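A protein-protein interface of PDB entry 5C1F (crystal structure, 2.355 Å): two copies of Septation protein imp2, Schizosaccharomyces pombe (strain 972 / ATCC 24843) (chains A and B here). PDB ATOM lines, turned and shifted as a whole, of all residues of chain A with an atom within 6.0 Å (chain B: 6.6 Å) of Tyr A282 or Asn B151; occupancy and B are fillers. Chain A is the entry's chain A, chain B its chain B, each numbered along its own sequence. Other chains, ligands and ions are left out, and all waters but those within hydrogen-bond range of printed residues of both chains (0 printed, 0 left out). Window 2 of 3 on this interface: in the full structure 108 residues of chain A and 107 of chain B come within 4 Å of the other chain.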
ATOM      1  N   PHE A 279      28.130   7.611  18.990  1.00  0.00           N
ATOM      2  CA  PHE A 279      28.106   6.253  19.518  1.00  0.00           C
ATOM      3  C   PHE A 279      27.423   5.300  18.543  1.00  0.00           C
ATOM      4  O   PHE A 279      26.326   5.577  18.057  1.00  0.00           O
ATOM      5  CB  PHE A 279      27.393   6.229  20.872  1.00  0.00           C
ATOM      6  CG  PHE A 279      27.322   4.865  21.502  1.00  0.00           C
ATOM      7  CD1 PHE A 279      28.377   4.379  22.256  1.00  0.00           C
ATOM      8  CD2 PHE A 279      26.193   4.077  21.354  1.00  0.00           C
ATOM      9  CE1 PHE A 279      28.310   3.129  22.844  1.00  0.00           C
ATOM     10  CE2 PHE A 279      26.122   2.826  21.938  1.00  0.00           C
ATOM     11  CZ  PHE A 279      27.182   2.352  22.683  1.00  0.00           C
ATOM     12  N   TYR A 280      28.075   4.175  18.259  1.00  0.00           N
ATOM     13  CA  TYR A 280      27.514   3.178  17.353  1.00  0.00           C
ATOM     14  C   TYR A 280      27.142   1.900  18.096  1.00  0.00           C
ATOM     15  O   TYR A 280      27.995   1.048  18.356  1.00  0.00           O
ATOM     16  CB  TYR A 280      28.495   2.868  16.222  1.00  0.00           C
ATOM     17  CG  TYR A 280      28.598   3.970  15.194  1.00  0.00           C
ATOM     18  CD1 TYR A 280      27.692   4.051  14.145  1.00  0.00           C
ATOM     19  CD2 TYR A 280      29.596   4.931  15.272  1.00  0.00           C
ATOM     20  CE1 TYR A 280      27.778   5.055  13.200  1.00  0.00           C
ATOM     21  CE2 TYR A 280      29.691   5.942  14.331  1.00  0.00           C
ATOM     22  CZ  TYR A 280      28.780   5.999  13.298  1.00  0.00           C
ATOM     23  OH  TYR A 280      28.869   7.003  12.358  1.00  0.00           O
ATOM     24  N   ASP A 281      25.862   1.780  18.432  1.00  0.00           N
ATOM     25  CA  ASP A 281      25.354   0.622  19.158  1.00  0.00           C
ATOM     26  C   ASP A 281      25.269  -0.596  18.246  1.00  0.00           C
ATOM     27  O   ASP A 281      24.460  -0.633  17.321  1.00  0.00           O
ATOM     28  CB  ASP A 281      23.982   0.928  19.761  1.00  0.00           C
ATOM     29  CG  ASP A 281      23.531  -0.126  20.755  1.00  0.00           C
ATOM     30  OD1 ASP A 281      23.083  -1.207  20.320  1.00  0.00           O
ATOM     31  OD2 ASP A 281      23.617   0.129  21.976  1.00  0.00           O
ATOM     32  N   TYR A 282      26.098  -1.596  18.529  1.00  0.00           N
ATOM     33  CA  TYR A 282      26.186  -2.804  17.711  1.00  0.00           C
ATOM     34  C   TYR A 282      24.842  -3.512  17.501  1.00  0.00           C
ATOM     35  O   TYR A 282      24.648  -4.200  16.498  1.00  0.00           O
ATOM     36  CB  TYR A 282      27.190  -3.778  18.342  1.00  0.00           C
ATOM     37  CG  TYR A 282      27.185  -5.165  17.735  1.00  0.00           C
ATOM     38  CD1 TYR A 282      27.874  -5.434  16.559  1.00  0.00           C
ATOM     39  CD2 TYR A 282      26.496  -6.207  18.344  1.00  0.00           C
ATOM     40  CE1 TYR A 282      27.870  -6.701  16.004  1.00  0.00           C
ATOM     41  CE2 TYR A 282      26.486  -7.476  17.795  1.00  0.00           C
ATOM     42  CZ  TYR A 282      27.175  -7.718  16.626  1.00  0.00           C
ATOM     43  OH  TYR A 282      27.167  -8.981  16.079  1.00  0.00           O
ATOM     44  N   TYR A 283      23.913  -3.327  18.433  1.00  0.00           N
ATOM     45  CA  TYR A 283      22.673  -4.102  18.439  1.00  0.00           C
ATOM     46  C   TYR A 283      21.534  -3.480  17.627  1.00  0.00           C
ATOM     47  O   TYR A 283      20.721  -4.200  17.047  1.00  0.00           O
ATOM     48  CB  TYR A 283      22.219  -4.329  19.882  1.00  0.00           C
ATOM     49  CG  TYR A 283      23.204  -5.147  20.687  1.00  0.00           C
ATOM     50  CD1 TYR A 283      23.117  -6.531  20.722  1.00  0.00           C
ATOM     51  CD2 TYR A 283      24.229  -4.538  21.398  1.00  0.00           C
ATOM     52  CE1 TYR A 283      24.016  -7.287  21.450  1.00  0.00           C
ATOM     53  CE2 TYR A 283      25.135  -5.285  22.130  1.00  0.00           C
ATOM     54  CZ  TYR A 283      25.023  -6.660  22.153  1.00  0.00           C
ATOM     55  OH  TYR A 283      25.920  -7.409  22.877  1.00  0.00           O
ATOM     56  N   LYS A 284      21.479  -2.153  17.573  1.00  0.00           N
ATOM     57  CA  LYS A 284      20.462  -1.461  16.781  1.00  0.00           C
ATOM     58  C   LYS A 284      20.905  -1.390  15.310  1.00  0.00           C
ATOM     59  O   LYS A 284      20.513  -0.496  14.559  1.00  0.00           O
ATOM     60  CB  LYS A 284      20.190  -0.063  17.366  1.00  0.00           C
ATOM     61  CG  LYS A 284      18.977   0.681  16.790  1.00  0.00           C
ATOM     62  CD  LYS A 284      17.802  -0.244  16.510  1.00  0.00           C
ATOM     63  CE  LYS A 284      16.715   0.479  15.721  1.00  0.00           C
ATOM     64  NZ  LYS A 284      15.583  -0.411  15.337  1.00  0.00           N
ATOM     65  N   GLY A 285      21.724  -2.356  14.907  1.00  0.00           N
ATOM     66  CA  GLY A 285      22.210  -2.445  13.541  1.00  0.00           C
ATOM     67  C   GLY A 285      23.268  -1.417  13.189  1.00  0.00           C
ATOM     68  O   GLY A 285      23.789  -1.415  12.071  1.00  0.00           O
ATOM     69  N   GLU A 286      23.590  -0.546  14.143  1.00  0.00           N
ATOM     70  CA  GLU A 286      24.537   0.538  13.908  1.00  0.00           C
ATOM     71  C   GLU A 286      25.939  -0.009  13.669  1.00  0.00           C
ATOM     72  O   GLU A 286      26.348  -1.003  14.271  1.00  0.00           O
ATOM     73  CB  GLU A 286      24.532   1.524  15.083  1.00  0.00           C
ATOM     74  CG  GLU A 286      23.138   1.803  15.633  1.00  0.00           C
ATOM     75  CD  GLU A 286      22.934   3.249  16.040  1.00  0.00           C
ATOM     76  OE1 GLU A 286      23.766   3.783  16.806  1.00  0.00           O
ATOM     77  OE2 GLU A 286      21.933   3.848  15.587  1.00  0.00           O
ATOM     78  N   TYR B 143      35.088  -2.241  21.883  1.00  0.00           N
ATOM     79  CA  TYR B 143      33.673  -2.572  22.020  1.00  0.00           C
ATOM     80  C   TYR B 143      33.187  -3.506  20.914  1.00  0.00           C
ATOM     81  O   TYR B 143      32.528  -4.509  21.187  1.00  0.00           O
ATOM     82  CB  TYR B 143      32.831  -1.296  22.035  1.00  0.00           C
ATOM     83  CG  TYR B 143      31.341  -1.528  21.915  1.00  0.00           C
ATOM     84  CD1 TYR B 143      30.619  -2.100  22.955  1.00  0.00           C
ATOM     85  CD2 TYR B 143      30.654  -1.162  20.764  1.00  0.00           C
ATOM     86  CE1 TYR B 143      29.254  -2.310  22.847  1.00  0.00           C
ATOM     87  CE2 TYR B 143      29.291  -1.367  20.648  1.00  0.00           C
ATOM     88  CZ  TYR B 143      28.596  -1.940  21.691  1.00  0.00           C
ATOM     89  OH  TYR B 143      27.238  -2.143  21.577  1.00  0.00           O
ATOM     90  N   HIS B 144      33.511  -3.183  19.665  1.00  0.00           N
ATOM     91  CA  HIS B 144      33.036  -3.980  18.537  1.00  0.00           C
ATOM     92  C   HIS B 144      33.799  -5.292  18.389  1.00  0.00           C
ATOM     93  O   HIS B 144      33.275  -6.261  17.839  1.00  0.00           O
ATOM     94  CB  HIS B 144      33.107  -3.174  17.240  1.00  0.00           C
ATOM     95  CG  HIS B 144      31.855  -2.409  16.940  1.00  0.00           C
ATOM     96  ND1 HIS B 144      30.754  -2.989  16.346  1.00  0.00           N
ATOM     97  CD2 HIS B 144      31.530  -1.113  17.150  1.00  0.00           C
ATOM     98  CE1 HIS B 144      29.804  -2.083  16.203  1.00  0.00           C
ATOM     99  NE2 HIS B 144      30.250  -0.935  16.683  1.00  0.00           N
ATOM    100  N   LEU B 146      34.656  -7.073  20.965  1.00  0.00           N
ATOM    101  CA  LEU B 146      33.996  -7.926  21.945  1.00  0.00           C
ATOM    102  C   LEU B 146      32.632  -8.379  21.431  1.00  0.00           C
ATOM    103  O   LEU B 146      32.225  -9.521  21.649  1.00  0.00           O
ATOM    104  CB  LEU B 146      33.843  -7.196  23.280  1.00  0.00           C
ATOM    105  CG  LEU B 146      35.125  -6.894  24.057  1.00  0.00           C
ATOM    106  CD1 LEU B 146      34.804  -6.131  25.333  1.00  0.00           C
ATOM    107  CD2 LEU B 146      35.877  -8.177  24.370  1.00  0.00           C
ATOM    108  N   CYS B 147      31.934  -7.475  20.747  1.00  0.00           N
ATOM    109  CA  CYS B 147      30.633  -7.782  20.163  1.00  0.00           C
ATOM    110  C   CYS B 147      30.749  -8.860  19.093  1.00  0.00           C
ATOM    111  O   CYS B 147      29.864  -9.706  18.954  1.00  0.00           O
ATOM    112  CB  CYS B 147      29.996  -6.522  19.569  1.00  0.00           C
ATOM    113  SG  CYS B 147      29.420  -5.322  20.791  1.00  0.00           S
ATOM    114  N   LYS B 148      31.844  -8.825  18.337  1.00  0.00           N
ATOM    115  CA  LYS B 148      32.087  -9.840  17.321  1.00  0.00           C
ATOM    116  C   LYS B 148      32.466 -11.162  17.983  1.00  0.00           C
ATOM    117  O   LYS B 148      32.272 -12.231  17.406  1.00  0.00           O
ATOM    118  CB  LYS B 148      33.186  -9.397  16.347  1.00  0.00           C
ATOM    119  CG  LYS B 148      34.582  -9.891  16.712  1.00  0.00           C
ATOM    120  CD  LYS B 148      35.554  -9.791  15.546  1.00  0.00           C
ATOM    121  CE  LYS B 148      35.957  -8.354  15.266  1.00  0.00           C
ATOM    122  NZ  LYS B 148      37.004  -8.277  14.209  1.00  0.00           N
ATOM    123  N   LYS B 149      32.998 -11.088  19.200  1.00  0.00           N
ATOM    124  CA  LYS B 149      33.488 -12.281  19.878  1.00  0.00           C
ATOM    125  C   LYS B 149      32.365 -12.987  20.625  1.00  0.00           C
ATOM    126  O   LYS B 149      32.328 -14.218  20.689  1.00  0.00           O
ATOM    127  CB  LYS B 149      34.627 -11.930  20.836  1.00  0.00           C
ATOM    128  CG  LYS B 149      35.798 -12.893  20.750  1.00  0.00           C
ATOM    129  CD  LYS B 149      36.174 -13.150  19.295  1.00  0.00           C
ATOM    130  CE  LYS B 149      37.148 -14.314  19.157  1.00  0.00           C
ATOM    131  NZ  LYS B 149      37.328 -14.719  17.729  1.00  0.00           N
ATOM    132  N   VAL B 150      31.454 -12.204  21.193  1.00  0.00           N
ATOM    133  CA  VAL B 150      30.242 -12.751  21.787  1.00  0.00           C
ATOM    134  C   VAL B 150      29.428 -13.425  20.683  1.00  0.00           C
ATOM    135  O   VAL B 150      28.802 -14.469  20.895  1.00  0.00           O
ATOM    136  CB  VAL B 150      29.417 -11.653  22.496  1.00  0.00           C
ATOM    137  CG1 VAL B 150      27.919 -11.888  22.334  1.00  0.00           C
ATOM    138  CG2 VAL B 150      29.800 -11.570  23.965  1.00  0.00           C
ATOM    139  N   ASN B 151      29.474 -12.825  19.496  1.00  0.00           N
ATOM    140  CA  ASN B 151      28.811 -13.363  18.315  1.00  0.00           C
ATOM    141  C   ASN B 151      29.436 -14.676  17.855  1.00  0.00           C
ATOM    142  O   ASN B 151      28.751 -15.526  17.291  1.00  0.00           O
ATOM    143  CB  ASN B 151      28.851 -12.340  17.176  1.00  0.00           C
ATOM    144  CG  ASN B 151      27.619 -12.400  16.293  1.00  0.00           C
ATOM    145  OD1 ASN B 151      26.660 -11.657  16.500  1.00  0.00           O
ATOM    146  ND2 ASN B 151      27.642 -13.280  15.298  1.00  0.00           N
ATOM    147  N   TYR B 152      30.737 -14.834  18.084  1.00  0.00           N
ATOM    148  CA  TYR B 152      31.426 -16.072  17.722  1.00  0.00           C
ATOM    149  C   TYR B 152      30.966 -17.223  18.616  1.00  0.00           C
ATOM    150  O   TYR B 152      30.564 -18.279  18.120  1.00  0.00           O
ATOM    151  CB  TYR B 152      32.947 -15.910  17.822  1.00  0.00           C
ATOM    152  CG  TYR B 152      33.755 -17.091  17.298  1.00  0.00           C
ATOM    153  CD1 TYR B 152      33.217 -17.984  16.375  1.00  0.00           C
ATOM    154  CD2 TYR B 152      35.059 -17.312  17.731  1.00  0.00           C
ATOM    155  CE1 TYR B 152      33.957 -19.060  15.898  1.00  0.00           C
ATOM    156  CE2 TYR B 152      35.804 -18.385  17.258  1.00  0.00           C
ATOM    157  CZ  TYR B 152      35.248 -19.254  16.343  1.00  0.00           C
ATOM    158  OH  TYR B 152      35.980 -20.320  15.870  1.00  0.00           O
ATOM    159  N   TYR B 153      31.025 -17.016  19.928  1.00  0.00           N
ATOM    160  CA  TYR B 153      30.672 -18.058  20.885  1.00  0.00           C
ATOM    161  C   TYR B 153      29.193 -18.422  20.797  1.00  0.00           C
ATOM    162  O   TYR B 153      28.807 -19.561  21.064  1.00  0.00           O
ATOM    163  CB  TYR B 153      31.031 -17.614  22.306  1.00  0.00           C
ATOM    164  CG  TYR B 153      32.504 -17.329  22.503  1.00  0.00           C
ATOM    165  CD1 TYR B 153      33.470 -18.107  21.880  1.00  0.00           C
ATOM    166  CD2 TYR B 153      32.928 -16.276  23.302  1.00  0.00           C
ATOM    167  CE1 TYR B 153      34.818 -17.850  22.052  1.00  0.00           C
ATOM    168  CE2 TYR B 153      34.277 -16.009  23.480  1.00  0.00           C
ATOM    169  CZ  TYR B 153      35.217 -16.800  22.851  1.00  0.00           C
ATOM    170  OH  TYR B 153      36.559 -16.544  23.023  1.00  0.00           O
ATOM    171  N   VAL B 154      28.372 -17.449  20.415  1.00  0.00           N
ATOM    172  CA  VAL B 154      26.938 -17.670  20.269  1.00  0.00           C
ATOM    173  C   VAL B 154      26.609 -18.571  19.074  1.00  0.00           C
ATOM    174  O   VAL B 154      25.818 -19.509  19.195  1.00  0.00           O
ATOM    175  CB  VAL B 154      26.182 -16.327  20.130  1.00  0.00           C
ATOM    176  CG1 VAL B 154      24.875 -16.516  19.374  1.00  0.00           C
ATOM    177  CG2 VAL B 154      25.930 -15.710  21.501  1.00  0.00           C
ATOM    178  N   SER B 155      27.227 -18.295  17.928  1.00  0.00           N
ATOM    179  CA  SER B 155      26.991 -19.088  16.723  1.00  0.00           C
ATOM    180  C   SER B 155      27.522 -20.516  16.867  1.00  0.00           C
ATOM    181  O   SER B 155      27.123 -21.414  16.123  1.00  0.00           O
ATOM    182  CB  SER B 155      27.628 -18.413  15.503  1.00  0.00           C
ATOM    183  OG  SER B 155      29.032 -18.305  15.653  1.00  0.00           O
ATOM    184  N   GLN B 156      28.416 -20.719  17.830  1.00  0.00           N
ATOM    185  CA  GLN B 156      29.003 -22.033  18.077  1.00  0.00           C
ATOM    186  C   GLN B 156      28.284 -22.785  19.196  1.00  0.00           C
ATOM    187  O   GLN B 156      28.672 -23.899  19.553  1.00  0.00           O
ATOM    188  CB  GLN B 156      30.490 -21.898  18.419  1.00  0.00           C
ATOM    189  CG  GLN B 156      31.389 -21.605  17.230  1.00  0.00           C
ATOM    190  CD  GLN B 156      32.355 -22.738  16.950  1.00  0.00           C
ATOM    191  OE1 GLN B 156      32.188 -23.847  17.458  1.00  0.00           O
ATOM    192  NE2 GLN B 156      33.376 -22.465  16.146  1.00  0.00           N
ATOM    193  N   ILE B 179      31.431  -6.735  27.684  1.00  0.00           N
ATOM    194  CA  ILE B 179      30.775  -5.899  26.679  1.00  0.00           C
ATOM    195  C   ILE B 179      30.041  -4.714  27.306  1.00  0.00           C
ATOM    196  O   ILE B 179      30.156  -3.582  26.827  1.00  0.00           O
ATOM    197  CB  ILE B 179      29.779  -6.721  25.825  1.00  0.00           C
ATOM    198  CG1 ILE B 179      30.509  -7.423  24.677  1.00  0.00           C
ATOM    199  CG2 ILE B 179      28.671  -5.835  25.271  1.00  0.00           C
ATOM    200  CD1 ILE B 179      29.584  -7.984  23.617  1.00  0.00           C
ATOM    201  N   TYR B 186      33.132   3.227  25.909  1.00  0.00           N
ATOM    202  CA  TYR B 186      32.898   3.738  24.565  1.00  0.00           C
ATOM    203  C   TYR B 186      32.053   5.010  24.637  1.00  0.00           C
ATOM    204  O   TYR B 186      32.404   6.026  24.038  1.00  0.00           O
ATOM    205  CB  TYR B 186      32.212   2.664  23.707  1.00  0.00           C
ATOM    206  CG  TYR B 186      32.001   3.002  22.238  1.00  0.00           C
ATOM    207  CD1 TYR B 186      32.596   4.112  21.650  1.00  0.00           C
ATOM    208  CD2 TYR B 186      31.194   2.196  21.443  1.00  0.00           C
ATOM    209  CE1 TYR B 186      32.389   4.410  20.314  1.00  0.00           C
ATOM    210  CE2 TYR B 186      30.982   2.485  20.110  1.00  0.00           C
ATOM    211  CZ  TYR B 186      31.580   3.590  19.550  1.00  0.00           C
ATOM    212  OH  TYR B 186      31.367   3.873  18.220  1.00  0.00           O
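OG of Ser B155 lies within hydrogen-bond range of O of Asn B151 (3.2 Å). SG of Cys B147 is in hydrogen-bond range of O of Tyr B143. OD1 of Asp A281 is in hydrogen-bond range of N of Tyr A283 (3.0 Å).
Printed residues of chain B within 4 Å of Phe A279: Tyr B186 (3.3 Å). Of chain B, only Tyr B143, His B144, Cys B147 and Asn B151 come within 4 Å of Tyr A282. Of the printed residues of chain A, Tyr B143 touches Tyr A280 (3.6 Å), Tyr A282 (3.3 Å) and Tyr A283 (3.8 Å). Printed residues of chain A within 4 Å of Cys B147: Tyr A282. Of the printed residues of chain A, Asn B151 touches Tyr A282. Val B154 touches none of the printed residues of chain A. Of the printed residues of chain A, Ile B179 touches Tyr A283 (3.8 Å). Of the printed residues of chain A, Tyr B186 touches Phe A279 (3.3 Å) and Tyr A280 (3.3 Å). The nearest residue of chain B that does not touch Tyr A282 is Lys B148 (5.1 Å). The nearest printed residue of chain A that does not touch Asn B151 is Tyr A283 (7.1 Å).
Of the 15 printed residues of chain B, 6 touch a printed residue of chain A. Hydrophobic or aromatic side chains of chain B within 4 Å of the printed part of chain A: Tyr B143, His B144, Ile B179 and Tyr B186. Of the 8 printed residues of chain A, 4 touch a printed residue of chain B. Hydrophobic or aromatic side chains of chain A within 4 Å of the printed part of chain B: Phe A279, Tyr A280, Tyr A282 and Tyr A283. Among the printed residues, no Asp or Glu carboxylate lies within 4 Å of a Lys or Arg side-chain nitrogen of the other chain.
CD2 of Tyr B186 touches CE1 of Phe A279 (3.3 Å). Tyr A280 touches Tyr B143. CB of Tyr A282 touches CE1 of His B144, at 3.8 Å. Cys B147 touches Tyr A282 (CB to CG, 3.6 Å). CE2 of Tyr A283 touches OH of Tyr B143 (3.8 Å). Ile B179 touches Tyr A283.
No position is printed for both chains. Of the 10 pairs that touch across the chains among the printed residues, none has its exchanged pair printed and touching as well.
OH of Tyr B186 lies within hydrogen-bond range of N of Tyr A280 (3.3 Å). The backbone NH (N) of Tyr A282 lies within hydrogen-bond range of the side-chain hydroxyl (OH) of Tyr B143 (3.3 Å). A ring nitrogen (NE2) of His B144 is in hydrogen-bond range of the backbone carbonyl oxygen (O) of Tyr A280, 3.4 Å away. The side-chain hydroxyl of Tyr A282 is in hydrogen-bond range of the side-chain amide oxygen of Asn B151, at 2.8 Å.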
